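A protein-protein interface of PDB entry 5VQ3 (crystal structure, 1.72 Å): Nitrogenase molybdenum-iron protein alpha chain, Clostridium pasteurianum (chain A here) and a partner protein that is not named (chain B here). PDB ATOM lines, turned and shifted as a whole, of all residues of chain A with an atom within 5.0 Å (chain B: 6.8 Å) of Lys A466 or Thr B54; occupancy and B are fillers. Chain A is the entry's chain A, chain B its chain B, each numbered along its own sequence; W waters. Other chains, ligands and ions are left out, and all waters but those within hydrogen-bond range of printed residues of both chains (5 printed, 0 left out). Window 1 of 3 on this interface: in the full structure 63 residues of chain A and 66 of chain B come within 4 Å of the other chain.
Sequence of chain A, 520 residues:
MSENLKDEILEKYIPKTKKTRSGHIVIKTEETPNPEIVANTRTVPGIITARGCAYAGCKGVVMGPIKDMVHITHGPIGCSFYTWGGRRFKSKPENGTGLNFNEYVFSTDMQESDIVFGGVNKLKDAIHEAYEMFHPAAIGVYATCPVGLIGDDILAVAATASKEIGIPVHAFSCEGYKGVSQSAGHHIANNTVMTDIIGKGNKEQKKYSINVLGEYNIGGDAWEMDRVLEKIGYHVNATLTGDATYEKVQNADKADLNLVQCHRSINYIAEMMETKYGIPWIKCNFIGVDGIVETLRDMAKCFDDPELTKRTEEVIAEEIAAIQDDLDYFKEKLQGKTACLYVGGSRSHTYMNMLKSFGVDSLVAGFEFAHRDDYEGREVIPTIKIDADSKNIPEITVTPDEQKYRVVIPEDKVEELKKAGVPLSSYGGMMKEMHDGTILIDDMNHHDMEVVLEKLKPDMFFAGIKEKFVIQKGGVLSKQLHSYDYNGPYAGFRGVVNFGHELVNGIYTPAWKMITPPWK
Printed residues of chain A that touch a printed residue of chain B: Thr A49, Ala A50, Ile A465, Lys A466, Phe A469 and Val A470.
Among the printed residues, 13 pairs touch across the chains.
The side-chain amino group (NZ) of Lys A466 lies within hydrogen-bond range of the side-chain hydroxyl (OG) of Ser B50, 3.1 Å away.
NH1 of Arg B53 touches O of Thr A49, 3.6 Å away.
Ile A465 touches Thr B54.
Ile A465 touches Ser B57 (O to CB, 3.97 Å).
Ile A465 touches Arg B58.
Lys A466 touches Arg B53.
OG1 of Thr B54 touches CG of Lys A466, 3.4 Å away.
Phe A469 touches Glu B62.
Pro B63 touches Phe A469.
Val A470 touches Pro B63.
Met B65 touches Val A470 (CE to CG2, 3.5 Å).
OG1 of Thr B54 sits at hydrogen-bond distance from O of Ser B50, 2.7 Å away.
NE of Arg B53 lies within hydrogen-bond range of O of Ala B64, at 2.9 Å.
The backbone carbonyl oxygen (O) of Glu B62 is in hydrogen-bond range of the side-chain hydroxyl (OG) of Ser B57.
NZ of Lys A466 sits at hydrogen-bond distance from O of Ala A50, at 3.1 Å.
Printed residues of chain B within 4 Å of Phe A469: Ser B57 (3.8 Å), Glu B62 (3.6 Å) and Pro B63 (3.6 Å).
Printed residues of chain A within 4 Å of Ser B50: Ala A50 and Lys A466.
Printed residues of chain A within 4 Å of Arg B53: Thr A49 (3.6 Å) and Lys A466 (3.8 Å).
Of the printed residues of chain A, Thr B54 touches Ile A465 (3.5 Å) and Lys A466 (3.4 Å).
The nearest printed residue of chain A that does not touch Thr B54 is Ala A50 (7.1 Å).
Water W2 lies within hydrogen-bond range of the backbone carbonyl oxygen of Lys A466 (2.7 Å), the backbone NH of Ala B64 (2.9 Å) and the guanidinium group of Arg B53 (3.1 Å).
Water W5 lies within hydrogen-bond range of the side-chain hydroxyl of Thr B54 (2.7 Å), the side-chain amino group of Lys A466 (2.9 Å) and the side-chain hydroxyl of Ser B50 (3.2 Å).
Water W4 lies within hydrogen-bond range of the backbone carbonyl oxygen of Thr A49, the guanidinium group of Arg B53 and the side-chain sulfur of Cys B49.
Water W1 lies within hydrogen-bond range of O of Ala A50 (2.9 Å) and OG of Ser B50 (3.0 Å).
Water W3 lies within hydrogen-bond range of NH1 of Arg B53 and OE2 of Glu A467.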
ATOM      1  N   THR A  49     -36.521  -9.359 -20.263  1.00  0.00           N
ATOM      2  CA  THR A  49     -35.975  -8.525 -19.211  1.00  0.00           C
ATOM      3  C   THR A  49     -34.451  -8.421 -19.391  1.00  0.00           C
ATOM      4  O   THR A  49     -33.851  -9.229 -20.094  1.00  0.00           O
ATOM      5  CB  THR A  49     -36.263  -9.169 -17.845  1.00  0.00           C
ATOM      6  OG1 THR A  49     -35.775  -8.363 -16.767  1.00  0.00           O
ATOM      7  CG2 THR A  49     -35.623 -10.555 -17.761  1.00  0.00           C
ATOM      8  N   ALA A  50     -33.825  -7.464 -18.722  1.00  0.00           N
ATOM      9  CA  ALA A  50     -32.357  -7.432 -18.673  1.00  0.00           C
ATOM     10  C   ALA A  50     -31.852  -7.895 -17.325  1.00  0.00           C
ATOM     11  O   ALA A  50     -30.645  -7.952 -17.122  1.00  0.00           O
ATOM     12  CB  ALA A  50     -31.866  -6.012 -18.933  1.00  0.00           C
ATOM     13  N   GLU A 368     -33.548  -1.740 -14.061  1.00  0.00           N
ATOM     14  CA  GLU A 368     -33.844  -3.157 -13.983  1.00  0.00           C
ATOM     15  C   GLU A 368     -34.521  -3.530 -12.663  1.00  0.00           C
ATOM     16  O   GLU A 368     -35.483  -4.309 -12.658  1.00  0.00           O
ATOM     17  CB  GLU A 368     -32.580  -4.005 -14.102  1.00  0.00           C
ATOM     18  CG  GLU A 368     -31.826  -3.874 -15.404  1.00  0.00           C
ATOM     19  CD  GLU A 368     -30.511  -4.693 -15.464  1.00  0.00           C
ATOM     20  OE1 GLU A 368     -29.684  -4.405 -16.397  1.00  0.00           O
ATOM     21  OE2 GLU A 368     -30.319  -5.618 -14.634  1.00  0.00           O
ATOM     22  N   GLY A 464     -26.857  -1.215 -21.394  1.00  0.00           N
ATOM     23  CA  GLY A 464     -25.841  -2.233 -21.130  1.00  0.00           C
ATOM     24  C   GLY A 464     -25.552  -3.003 -22.413  1.00  0.00           C
ATOM     25  O   GLY A 464     -25.936  -2.586 -23.510  1.00  0.00           O
ATOM     26  N   ILE A 465     -24.802  -4.090 -22.277  1.00  0.00           N
ATOM     27  CA  ILE A 465     -24.279  -4.835 -23.406  1.00  0.00           C
ATOM     28  C   ILE A 465     -25.389  -5.569 -24.207  1.00  0.00           C
ATOM     29  O   ILE A 465     -25.283  -5.698 -25.406  1.00  0.00           O
ATOM     30  CB  ILE A 465     -23.178  -5.824 -22.900  1.00  0.00           C
ATOM     31  CG1 ILE A 465     -22.431  -6.468 -24.054  1.00  0.00           C
ATOM     32  CG2 ILE A 465     -23.770  -6.900 -21.986  1.00  0.00           C
ATOM     33  CD1 ILE A 465     -21.685  -5.484 -24.912  1.00  0.00           C
ATOM     34  N   LYS A 466     -26.471  -5.976 -23.546  1.00  0.00           N
ATOM     35  CA  LYS A 466     -27.525  -6.742 -24.198  1.00  0.00           C
ATOM     36  C   LYS A 466     -28.326  -5.808 -25.118  1.00  0.00           C
ATOM     37  O   LYS A 466     -28.836  -6.234 -26.171  1.00  0.00           O
ATOM     38  CB  LYS A 466     -28.413  -7.462 -23.193  1.00  0.00           C
ATOM     39  CG  LYS A 466     -27.686  -8.532 -22.403  1.00  0.00           C
ATOM     40  CD  LYS A 466     -28.580  -9.454 -21.557  1.00  0.00           C
ATOM     41  CE  LYS A 466     -29.426  -8.725 -20.546  1.00  0.00           C
ATOM     42  NZ  LYS A 466     -28.723  -7.936 -19.505  1.00  0.00           N
ATOM     43  N   GLU A 467     -28.417  -4.530 -24.724  1.00  0.00           N
ATOM     44  CA  GLU A 467     -29.197  -3.558 -25.483  1.00  0.00           C
ATOM     45  C   GLU A 467     -28.358  -2.742 -26.461  1.00  0.00           C
ATOM     46  O   GLU A 467     -28.887  -2.233 -27.451  1.00  0.00           O
ATOM     47  CB  GLU A 467     -29.858  -2.582 -24.519  1.00  0.00           C
ATOM     48  CG  GLU A 467     -30.703  -3.189 -23.421  1.00  0.00           C
ATOM     49  CD  GLU A 467     -29.933  -3.769 -22.211  1.00  0.00           C
ATOM     50  OE1 GLU A 467     -28.761  -3.412 -21.935  1.00  0.00           O
ATOM     51  OE2 GLU A 467     -30.505  -4.655 -21.532  1.00  0.00           O
ATOM     52  N   LYS A 468     -27.061  -2.578 -26.185  1.00  0.00           N
ATOM     53  CA  LYS A 468     -26.231  -1.660 -26.978  1.00  0.00           C
ATOM     54  C   LYS A 468     -26.448  -1.879 -28.490  1.00  0.00           C
ATOM     55  O   LYS A 468     -26.679  -0.934 -29.226  1.00  0.00           O
ATOM     56  CB  LYS A 468     -24.765  -1.841 -26.665  1.00  0.00           C
ATOM     57  CG  LYS A 468     -23.833  -0.976 -27.491  1.00  0.00           C
ATOM     58  CD  LYS A 468     -22.352  -1.227 -27.169  1.00  0.00           C
ATOM     59  CE  LYS A 468     -21.402  -0.309 -27.942  1.00  0.00           C
ATOM     60  NZ  LYS A 468     -21.358   1.072 -27.403  1.00  0.00           N
ATOM     61  N   PHE A 469     -26.278  -3.098 -28.959  1.00  0.00           N
ATOM     62  CA  PHE A 469     -26.246  -3.342 -30.390  1.00  0.00           C
ATOM     63  C   PHE A 469     -27.639  -3.342 -31.002  1.00  0.00           C
ATOM     64  O   PHE A 469     -27.786  -3.004 -32.168  1.00  0.00           O
ATOM     65  CB  PHE A 469     -25.435  -4.627 -30.721  1.00  0.00           C
ATOM     66  CG  PHE A 469     -23.994  -4.553 -30.256  1.00  0.00           C
ATOM     67  CD1 PHE A 469     -23.126  -3.602 -30.782  1.00  0.00           C
ATOM     68  CD2 PHE A 469     -23.545  -5.346 -29.219  1.00  0.00           C
ATOM     69  CE1 PHE A 469     -21.835  -3.495 -30.329  1.00  0.00           C
ATOM     70  CE2 PHE A 469     -22.244  -5.236 -28.773  1.00  0.00           C
ATOM     71  CZ  PHE A 469     -21.404  -4.303 -29.307  1.00  0.00           C
ATOM     72  N   VAL A 470     -28.650  -3.705 -30.191  1.00  0.00           N
ATOM     73  CA  VAL A 470     -30.046  -3.541 -30.607  1.00  0.00           C
ATOM     74  C   VAL A 470     -30.348  -2.074 -30.942  1.00  0.00           C
ATOM     75  O   VAL A 470     -30.869  -1.754 -32.016  1.00  0.00           O
ATOM     76  CB  VAL A 470     -31.028  -3.969 -29.541  1.00  0.00           C
ATOM     77  CG1 VAL A 470     -32.421  -3.522 -29.970  1.00  0.00           C
ATOM     78  CG2 VAL A 470     -30.954  -5.478 -29.316  1.00  0.00           C
ATOM     79  N   MET B  29     -28.541 -22.017 -27.093  1.00  0.00           N
ATOM     80  CA  MET B  29     -28.969 -20.699 -27.561  1.00  0.00           C
ATOM     81  C   MET B  29     -28.397 -20.325 -28.921  1.00  0.00           C
ATOM     82  O   MET B  29     -29.100 -19.806 -29.786  1.00  0.00           O
ATOM     83  CB  MET B  29     -28.571 -19.641 -26.516  1.00  0.00           C
ATOM     84  CG  MET B  29     -29.045 -18.209 -26.832  1.00  0.00           C
ATOM     85  SD  MET B  29     -28.647 -17.077 -25.481  1.00  0.00           S
ATOM     86  CE  MET B  29     -29.715 -17.711 -24.177  1.00  0.00           C
ATOM     87  N   CYS B  48     -29.253 -16.867 -15.891  1.00  0.00           N
ATOM     88  CA  CYS B  48     -28.650 -17.688 -16.927  1.00  0.00           C
ATOM     89  C   CYS B  48     -28.814 -16.982 -18.288  1.00  0.00           C
ATOM     90  O   CYS B  48     -27.858 -16.722 -18.985  1.00  0.00           O
ATOM     91  CB  CYS B  48     -29.305 -19.064 -16.926  1.00  0.00           C
ATOM     92  SG  CYS B  48     -29.063 -19.953 -15.407  1.00  0.00           S
ATOM     93  N   CYS B  49     -30.053 -16.660 -18.630  1.00  0.00           N
ATOM     94  CA  CYS B  49     -30.370 -16.035 -19.904  1.00  0.00           C
ATOM     95  C   CYS B  49     -29.595 -14.743 -20.076  1.00  0.00           C
ATOM     96  O   CYS B  49     -29.001 -14.508 -21.111  1.00  0.00           O
ATOM     97  CB  CYS B  49     -31.860 -15.730 -19.964  1.00  0.00           C
ATOM     98  SG  CYS B  49     -32.448 -15.123 -21.558  1.00  0.00           S
ATOM     99  N   SER B  50     -29.549 -13.927 -19.047  1.00  0.00           N
ATOM    100  CA  SER B  50     -28.775 -12.701 -19.147  1.00  0.00           C
ATOM    101  C   SER B  50     -27.305 -12.949 -19.480  1.00  0.00           C
ATOM    102  O   SER B  50     -26.735 -12.325 -20.401  1.00  0.00           O
ATOM    103  CB  SER B  50     -28.847 -11.906 -17.878  1.00  0.00           C
ATOM    104  OG  SER B  50     -28.182 -10.672 -18.094  1.00  0.00           O
ATOM    105  N   TYR B  51     -26.677 -13.859 -18.738  1.00  0.00           N
ATOM    106  CA  TYR B  51     -25.274 -14.163 -18.934  1.00  0.00           C
ATOM    107  C   TYR B  51     -24.998 -14.774 -20.332  1.00  0.00           C
ATOM    108  O   TYR B  51     -24.010 -14.420 -20.998  1.00  0.00           O
ATOM    109  CB  TYR B  51     -24.773 -15.099 -17.842  1.00  0.00           C
ATOM    110  CG  TYR B  51     -24.413 -14.524 -16.485  1.00  0.00           C
ATOM    111  CD1 TYR B  51     -24.001 -13.219 -16.290  1.00  0.00           C
ATOM    112  CD2 TYR B  51     -24.422 -15.357 -15.389  1.00  0.00           C
ATOM    113  CE1 TYR B  51     -23.585 -12.779 -15.046  1.00  0.00           C
ATOM    114  CE2 TYR B  51     -24.019 -14.923 -14.155  1.00  0.00           C
ATOM    115  CZ  TYR B  51     -23.607 -13.629 -13.975  1.00  0.00           C
ATOM    116  OH  TYR B  51     -23.173 -13.224 -12.711  1.00  0.00           O
ATOM    117  N   HIS B  52     -25.917 -15.597 -20.824  1.00  0.00           N
ATOM    118  CA  HIS B  52     -25.717 -16.322 -22.056  1.00  0.00           C
ATOM    119  C   HIS B  52     -25.926 -15.403 -23.243  1.00  0.00           C
ATOM    120  O   HIS B  52     -25.157 -15.416 -24.202  1.00  0.00           O
ATOM    121  CB  HIS B  52     -26.601 -17.579 -22.090  1.00  0.00           C
ATOM    122  CG  HIS B  52     -26.349 -18.474 -20.916  1.00  0.00           C
ATOM    123  ND1 HIS B  52     -27.195 -19.483 -20.500  1.00  0.00           N
ATOM    124  CD2 HIS B  52     -25.330 -18.458 -20.034  1.00  0.00           C
ATOM    125  CE1 HIS B  52     -26.729 -20.017 -19.394  1.00  0.00           C
ATOM    126  NE2 HIS B  52     -25.594 -19.414 -19.094  1.00  0.00           N
ATOM    127  N   ARG B  53     -26.950 -14.578 -23.158  1.00  0.00           N
ATOM    128  CA  ARG B  53     -27.106 -13.514 -24.129  1.00  0.00           C
ATOM    129  C   ARG B  53     -25.877 -12.612 -24.157  1.00  0.00           C
ATOM    130  O   ARG B  53     -25.406 -12.248 -25.235  1.00  0.00           O
ATOM    131  CB  ARG B  53     -28.365 -12.677 -23.865  1.00  0.00           C
ATOM    132  CG  ARG B  53     -29.678 -13.411 -24.053  1.00  0.00           C
ATOM    133  CD  ARG B  53     -30.851 -12.511 -23.703  1.00  0.00           C
ATOM    134  NE  ARG B  53     -30.916 -11.344 -24.584  1.00  0.00           N
ATOM    135  CZ  ARG B  53     -31.429 -10.168 -24.253  1.00  0.00           C
ATOM    136  NH1 ARG B  53     -31.988  -9.955 -23.040  1.00  0.00           N
ATOM    137  NH2 ARG B  53     -31.396  -9.186 -25.153  1.00  0.00           N
ATOM    138  N   THR B  54     -25.373 -12.259 -22.983  1.00  0.00           N
ATOM    139  CA  THR B  54     -24.265 -11.305 -22.860  1.00  0.00           C
ATOM    140  C   THR B  54     -22.989 -11.820 -23.531  1.00  0.00           C
ATOM    141  O   THR B  54     -22.320 -11.072 -24.262  1.00  0.00           O
ATOM    142  CB  THR B  54     -24.026 -10.962 -21.403  1.00  0.00           C
ATOM    143  OG1 THR B  54     -25.150 -10.225 -20.926  1.00  0.00           O
ATOM    144  CG2 THR B  54     -22.751 -10.167 -21.177  1.00  0.00           C
ATOM    145  N   VAL B  55     -22.658 -13.086 -23.314  1.00  0.00           N
ATOM    146  CA  VAL B  55     -21.414 -13.594 -23.917  1.00  0.00           C
ATOM    147  C   VAL B  55     -21.492 -13.622 -25.445  1.00  0.00           C
ATOM    148  O   VAL B  55     -20.495 -13.321 -26.133  1.00  0.00           O
ATOM    149  CB  VAL B  55     -20.984 -14.935 -23.357  1.00  0.00           C
ATOM    150  CG1 VAL B  55     -21.903 -16.073 -23.816  1.00  0.00           C
ATOM    151  CG2 VAL B  55     -19.547 -15.196 -23.771  1.00  0.00           C
ATOM    152  N   LEU B  56     -22.682 -13.900 -25.965  1.00  0.00           N
ATOM    153  CA  LEU B  56     -22.859 -13.890 -27.409  1.00  0.00           C
ATOM    154  C   LEU B  56     -22.664 -12.468 -27.947  1.00  0.00           C
ATOM    155  O   LEU B  56     -22.013 -12.266 -28.997  1.00  0.00           O
ATOM    156  CB  LEU B  56     -24.195 -14.490 -27.831  1.00  0.00           C
ATOM    157  CG  LEU B  56     -24.334 -15.986 -27.596  1.00  0.00           C
ATOM    158  CD1 LEU B  56     -25.775 -16.430 -27.678  1.00  0.00           C
ATOM    159  CD2 LEU B  56     -23.416 -16.762 -28.517  1.00  0.00           C
ATOM    160  N   SER B  57     -23.224 -11.472 -27.259  1.00  0.00           N
ATOM    161  CA  SER B  57     -23.023 -10.075 -27.689  1.00  0.00           C
ATOM    162  C   SER B  57     -21.584  -9.620 -27.593  1.00  0.00           C
ATOM    163  O   SER B  57     -21.112  -8.844 -28.458  1.00  0.00           O
ATOM    164  CB  SER B  57     -23.914  -9.093 -26.952  1.00  0.00           C
ATOM    165  OG  SER B  57     -25.276  -9.275 -27.356  1.00  0.00           O
ATOM    166  N   ARG B  58     -20.889 -10.060 -26.545  1.00  0.00           N
ATOM    167  CA  ARG B  58     -19.500  -9.700 -26.385  1.00  0.00           C
ATOM    168  C   ARG B  58     -18.615 -10.298 -27.471  1.00  0.00           C
ATOM    169  O   ARG B  58     -17.606  -9.707 -27.874  1.00  0.00           O
ATOM    170  CB  ARG B  58     -19.026 -10.092 -25.007  1.00  0.00           C
ATOM    171  CG  ARG B  58     -19.602  -9.249 -23.869  1.00  0.00           C
ATOM    172  CD  ARG B  58     -19.170  -9.800 -22.505  1.00  0.00           C
ATOM    173  NE  ARG B  58     -19.557  -8.903 -21.423  1.00  0.00           N
ATOM    174  CZ  ARG B  58     -19.746  -9.235 -20.163  1.00  0.00           C
ATOM    175  NH1 ARG B  58     -19.585 -10.504 -19.758  1.00  0.00           N
ATOM    176  NH2 ARG B  58     -20.151  -8.284 -19.290  1.00  0.00           N
ATOM    177  N   HIS B  59     -18.974 -11.498 -27.928  1.00  0.00           N
ATOM    178  CA  HIS B  59     -18.198 -12.178 -28.955  1.00  0.00           C
ATOM    179  C   HIS B  59     -18.510 -11.584 -30.344  1.00  0.00           C
ATOM    180  O   HIS B  59     -17.628 -11.259 -31.110  1.00  0.00           O
ATOM    181  CB  HIS B  59     -18.505 -13.673 -28.940  1.00  0.00           C
ATOM    182  CG  HIS B  59     -17.871 -14.448 -30.049  1.00  0.00           C
ATOM    183  ND1 HIS B  59     -16.701 -15.173 -29.885  1.00  0.00           N
ATOM    184  CD2 HIS B  59     -18.218 -14.574 -31.352  1.00  0.00           C
ATOM    185  CE1 HIS B  59     -16.391 -15.753 -31.037  1.00  0.00           C
ATOM    186  NE2 HIS B  59     -17.291 -15.398 -31.946  1.00  0.00           N
ATOM    187  N   GLU B  62     -22.996  -7.974 -31.635  1.00  0.00           N
ATOM    188  CA  GLU B  62     -24.282  -8.077 -32.298  1.00  0.00           C
ATOM    189  C   GLU B  62     -25.321  -8.290 -31.219  1.00  0.00           C
ATOM    190  O   GLU B  62     -24.992  -8.770 -30.144  1.00  0.00           O
ATOM    191  CB  GLU B  62     -24.329  -9.263 -33.274  1.00  0.00           C
ATOM    192  CG  GLU B  62     -23.541  -9.046 -34.559  1.00  0.00           C
ATOM    193  CD  GLU B  62     -24.143  -7.963 -35.479  1.00  0.00           C
ATOM    194  OE1 GLU B  62     -25.117  -8.280 -36.203  1.00  0.00           O
ATOM    195  OE2 GLU B  62     -23.624  -6.826 -35.481  1.00  0.00           O
ATOM    196  N   PRO B  63     -26.598  -7.978 -31.514  1.00  0.00           N
ATOM    197  CA  PRO B  63     -27.654  -8.434 -30.596  1.00  0.00           C
ATOM    198  C   PRO B  63     -27.727  -9.952 -30.487  1.00  0.00           C
ATOM    199  O   PRO B  63     -27.380 -10.667 -31.444  1.00  0.00           O
ATOM    200  CB  PRO B  63     -28.963  -7.943 -31.285  1.00  0.00           C
ATOM    201  CG  PRO B  63     -28.549  -6.925 -32.278  1.00  0.00           C
ATOM    202  CD  PRO B  63     -27.165  -7.361 -32.725  1.00  0.00           C
ATOM    203  N   ALA B  64     -28.239 -10.436 -29.372  1.00  0.00           N
ATOM    204  CA  ALA B  64     -28.475 -11.862 -29.197  1.00  0.00           C
ATOM    205  C   ALA B  64     -29.703 -12.001 -28.335  1.00  0.00           C
ATOM    206  O   ALA B  64     -29.617 -11.915 -27.127  1.00  0.00           O
ATOM    207  CB  ALA B  64     -27.287 -12.539 -28.511  1.00  0.00           C
ATOM    208  N   MET B  65     -30.827 -12.153 -28.973  1.00  0.00           N
ATOM    209  CA  MET B  65     -32.086 -12.203 -28.293  1.00  0.00           C
ATOM    210  C   MET B  65     -32.482 -13.541 -27.715  1.00  0.00           C
ATOM    211  O   MET B  65     -32.317 -14.525 -28.344  1.00  0.00           O
ATOM    212  CB  MET B  65     -33.164 -11.889 -29.312  1.00  0.00           C
ATOM    213  CG  MET B  65     -33.344 -10.447 -29.662  1.00  0.00           C
ATOM    214  SD  MET B  65     -33.828  -9.463 -28.268  1.00  0.00           S
ATOM    215  CE  MET B  65     -32.341  -8.563 -28.279  1.00  0.00           C
ATOM    216  N   MET B 414     -13.643 -11.878 -27.340  1.00  0.00           N
ATOM    217  CA  MET B 414     -14.464 -10.729 -26.907  1.00  0.00           C
ATOM    218  C   MET B 414     -13.693  -9.427 -26.961  1.00  0.00           C
ATOM    219  O   MET B 414     -14.190  -8.385 -26.519  1.00  0.00           O
ATOM    220  CB  MET B 414     -14.967 -10.974 -25.480  1.00  0.00           C
ATOM    221  CG  MET B 414     -15.815 -12.241 -25.371  1.00  0.00           C
ATOM    222  SD  MET B 414     -16.457 -12.528 -23.718  1.00  0.00           S
ATOM    223  CE  MET B 414     -14.966 -12.977 -22.868  1.00  0.00           C
HETATM  224  O   HOH W   1     -28.073  -8.616 -15.901  1.00  0.00           O
HETATM  225  O   HOH W   2     -28.979  -8.744 -27.116  1.00  0.00           O
HETATM  226  O   HOH W   3     -32.355  -6.966 -22.601  1.00  0.00           O
HETATM  227  O   HOH W   4     -32.550 -11.651 -20.477  1.00  0.00           O
HETATM  228  O   HOH W   5     -25.923  -8.542 -18.910  1.00  0.00           O
